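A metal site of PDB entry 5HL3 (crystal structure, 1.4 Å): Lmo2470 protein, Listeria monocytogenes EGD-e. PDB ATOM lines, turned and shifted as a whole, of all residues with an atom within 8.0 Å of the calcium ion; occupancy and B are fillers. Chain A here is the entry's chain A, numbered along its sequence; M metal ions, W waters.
OD1 of Asn 165 lies within hydrogen-bond range of N of Gln 189, at 2.9 Å. The side-chain amide nitrogen (ND2) of Asn 167 lies within hydrogen-bond range of the backbone carbonyl oxygen (O) of Asn 165, 3.4 Å away. The side-chain amide nitrogen of Asn 167 lies within hydrogen-bond range of the side-chain carboxylate of Asp 141, 2.8 Å away.
Of the 11 residues printed, 3 come within 4 Å of the calcium ion.
The calcium ion is bound by OD1 of Asn 190, OD1 of Asn 167, OE1 of Gln 189, water W2, water W1 and water W3. The calcium ion has six donor atoms within binding distance.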
ATOM      1  N   ASP A 141      -9.442 -19.391 -30.217  1.00  0.00           N
ATOM      2  CA  ASP A 141      -9.396 -20.754 -29.709  1.00  0.00           C
ATOM      3  C   ASP A 141      -9.013 -21.603 -30.942  1.00  0.00           C
ATOM      4  O   ASP A 141      -9.867 -22.106 -31.647  1.00  0.00           O
ATOM      5  CB  ASP A 141     -10.737 -21.148 -29.104  1.00  0.00           C
ATOM      6  CG  ASP A 141     -10.713 -22.485 -28.407  1.00  0.00           C
ATOM      7  OD1 ASP A 141      -9.623 -23.028 -28.142  1.00  0.00           O
ATOM      8  OD2 ASP A 141     -11.824 -23.025 -28.153  1.00  0.00           O
ATOM      9  N   ASN A 165      -9.876 -20.659 -22.983  1.00  0.00           N
ATOM     10  CA  ASN A 165      -9.446 -21.867 -22.318  1.00  0.00           C
ATOM     11  C   ASN A 165      -9.213 -22.875 -23.429  1.00  0.00           C
ATOM     12  O   ASN A 165     -10.064 -23.698 -23.770  1.00  0.00           O
ATOM     13  CB  ASN A 165     -10.523 -22.291 -21.319  1.00  0.00           C
ATOM     14  CG  ASN A 165     -10.011 -23.290 -20.317  1.00  0.00           C
ATOM     15  OD1 ASN A 165      -9.167 -24.104 -20.614  1.00  0.00           O
ATOM     16  ND2 ASN A 165     -10.523 -23.224 -19.100  1.00  0.00           N
ATOM     17  N   PHE A 166      -8.021 -22.791 -24.016  1.00  0.00           N
ATOM     18  CA  PHE A 166      -7.717 -23.464 -25.307  1.00  0.00           C
ATOM     19  C   PHE A 166      -8.158 -24.917 -25.407  1.00  0.00           C
ATOM     20  O   PHE A 166      -7.713 -25.759 -24.647  1.00  0.00           O
ATOM     21  CB  PHE A 166      -6.221 -23.427 -25.612  1.00  0.00           C
ATOM     22  CG  PHE A 166      -5.635 -22.046 -25.661  1.00  0.00           C
ATOM     23  CD1 PHE A 166      -5.856 -21.231 -26.764  1.00  0.00           C
ATOM     24  CD2 PHE A 166      -4.827 -21.575 -24.635  1.00  0.00           C
ATOM     25  CE1 PHE A 166      -5.300 -19.957 -26.841  1.00  0.00           C
ATOM     26  CE2 PHE A 166      -4.260 -20.297 -24.720  1.00  0.00           C
ATOM     27  CZ  PHE A 166      -4.499 -19.493 -25.817  1.00  0.00           C
ATOM     28  N   ASN A 167      -8.984 -25.229 -26.420  1.00  0.00           N
ATOM     29  CA  ASN A 167      -9.511 -26.589 -26.557  1.00  0.00           C
ATOM     30  C   ASN A 167      -8.766 -27.537 -27.464  1.00  0.00           C
ATOM     31  O   ASN A 167      -8.904 -28.733 -27.294  1.00  0.00           O
ATOM     32  CB  ASN A 167     -10.965 -26.507 -27.051  1.00  0.00           C
ATOM     33  CG  ASN A 167     -11.914 -26.049 -25.960  1.00  0.00           C
ATOM     34  OD1 ASN A 167     -12.163 -26.799 -25.041  1.00  0.00           O
ATOM     35  ND2 ASN A 167     -12.362 -24.790 -26.013  1.00  0.00           N
ATOM     36  N   ASN A 168      -7.993 -27.034 -28.408  1.00  0.00           N
ATOM     37  CA  ASN A 168      -7.502 -27.874 -29.509  1.00  0.00           C
ATOM     38  C   ASN A 168      -6.006 -27.804 -29.767  1.00  0.00           C
ATOM     39  O   ASN A 168      -5.553 -28.042 -30.904  1.00  0.00           O
ATOM     40  CB  ASN A 168      -8.261 -27.513 -30.792  1.00  0.00           C
ATOM     41  CG  ASN A 168      -9.748 -27.301 -30.567  1.00  0.00           C
ATOM     42  OD1 ASN A 168     -10.467 -28.232 -30.175  1.00  0.00           O
ATOM     43  ND2 ASN A 168     -10.218 -26.094 -30.812  1.00  0.00           N
ATOM     44  N   ASP A 187      -8.766 -21.809 -15.708  1.00  0.00           N
ATOM     45  CA  ASP A 187      -8.416 -23.107 -15.114  1.00  0.00           C
ATOM     46  C   ASP A 187      -8.254 -24.053 -16.325  1.00  0.00           C
ATOM     47  O   ASP A 187      -9.169 -24.791 -16.701  1.00  0.00           O
ATOM     48  CB  ASP A 187      -9.516 -23.556 -14.165  1.00  0.00           C
ATOM     49  CG  ASP A 187      -9.095 -24.736 -13.305  1.00  0.00           C
ATOM     50  OD1 ASP A 187      -7.989 -25.255 -13.525  1.00  0.00           O
ATOM     51  OD2 ASP A 187      -9.892 -25.104 -12.414  1.00  0.00           O
ATOM     52  N   PHE A 188      -7.074 -23.964 -16.954  1.00  0.00           N
ATOM     53  CA  PHE A 188      -6.891 -24.595 -18.272  1.00  0.00           C
ATOM     54  C   PHE A 188      -7.278 -26.065 -18.271  1.00  0.00           C
ATOM     55  O   PHE A 188      -6.759 -26.839 -17.505  1.00  0.00           O
ATOM     56  CB  PHE A 188      -5.455 -24.438 -18.735  1.00  0.00           C
ATOM     57  CG  PHE A 188      -5.088 -23.037 -19.141  1.00  0.00           C
ATOM     58  CD1 PHE A 188      -5.595 -22.469 -20.290  1.00  0.00           C
ATOM     59  CD2 PHE A 188      -4.205 -22.288 -18.380  1.00  0.00           C
ATOM     60  CE1 PHE A 188      -5.254 -21.180 -20.653  1.00  0.00           C
ATOM     61  CE2 PHE A 188      -3.853 -20.994 -18.750  1.00  0.00           C
ATOM     62  CZ  PHE A 188      -4.379 -20.452 -19.890  1.00  0.00           C
ATOM     63  N   GLN A 189      -8.194 -26.444 -19.147  1.00  0.00           N
ATOM     64  CA  GLN A 189      -8.725 -27.789 -19.197  1.00  0.00           C
ATOM     65  C   GLN A 189      -7.998 -28.763 -20.095  1.00  0.00           C
ATOM     66  O   GLN A 189      -7.990 -29.958 -19.807  1.00  0.00           O
ATOM     67  CB  GLN A 189     -10.192 -27.747 -19.709  1.00  0.00           C
ATOM     68  CG  GLN A 189     -11.179 -26.977 -18.846  1.00  0.00           C
ATOM     69  CD  GLN A 189     -12.593 -27.084 -19.380  1.00  0.00           C
ATOM     70  OE1 GLN A 189     -12.803 -27.425 -20.539  1.00  0.00           O
ATOM     71  NE2 GLN A 189     -13.567 -26.841 -18.515  1.00  0.00           N
ATOM     72  N   ASN A 190      -7.389 -28.284 -21.171  1.00  0.00           N
ATOM     73  CA  ASN A 190      -6.948 -29.179 -22.246  1.00  0.00           C
ATOM     74  C   ASN A 190      -5.538 -28.953 -22.709  1.00  0.00           C
ATOM     75  O   ASN A 190      -5.210 -29.278 -23.859  1.00  0.00           O
ATOM     76  CB  ASN A 190      -7.931 -29.040 -23.447  1.00  0.00           C
ATOM     77  CG  ASN A 190      -9.391 -29.218 -23.047  1.00  0.00           C
ATOM     78  OD1 ASN A 190     -10.183 -28.297 -23.183  1.00  0.00           O
ATOM     79  ND2 ASN A 190      -9.734 -30.380 -22.526  1.00  0.00           N
ATOM     80  N   ILE A 191      -4.697 -28.428 -21.833  1.00  0.00           N
ATOM     81  CA  ILE A 191      -3.246 -28.316 -22.149  1.00  0.00           C
ATOM     82  C   ILE A 191      -2.410 -29.024 -21.083  1.00  0.00           C
ATOM     83  O   ILE A 191      -1.531 -28.449 -20.434  1.00  0.00           O
ATOM     84  CB  ILE A 191      -2.804 -26.863 -22.405  1.00  0.00           C
ATOM     85  CG1 ILE A 191      -3.191 -25.923 -21.247  1.00  0.00           C
ATOM     86  CG2 ILE A 191      -3.369 -26.358 -23.738  1.00  0.00           C
ATOM     87  CD1 ILE A 191      -2.645 -24.520 -21.426  1.00  0.00           C
ATOM     88  N   GLN A 211      -6.730 -27.536 -12.210  1.00  0.00           N
ATOM     89  CA  GLN A 211      -7.264 -28.865 -12.255  1.00  0.00           C
ATOM     90  C   GLN A 211      -6.546 -29.850 -13.200  1.00  0.00           C
ATOM     91  O   GLN A 211      -6.702 -31.065 -13.057  1.00  0.00           O
ATOM     92  CB  GLN A 211      -8.778 -28.804 -12.623  1.00  0.00           C
ATOM     93  CG  GLN A 211      -9.054 -28.371 -14.045  1.00  0.00           C
ATOM     94  CD  GLN A 211     -10.486 -27.862 -14.285  1.00  0.00           C
ATOM     95  OE1 GLN A 211     -11.447 -28.347 -13.695  1.00  0.00           O
ATOM     96  NE2 GLN A 211     -10.617 -26.916 -15.209  1.00  0.00           N
HETATM   97 CA    CA M   1     -12.421 -27.773 -22.905  1.00  0.00          CA
HETATM   98  O   HOH W   1     -11.705 -25.497 -22.367  1.00  0.00           O
HETATM   99  O   HOH W   2     -14.790 -27.210 -23.084  1.00  0.00           O
HETATM  100  O   HOH W   3     -13.073 -29.464 -24.601  1.00  0.00           O
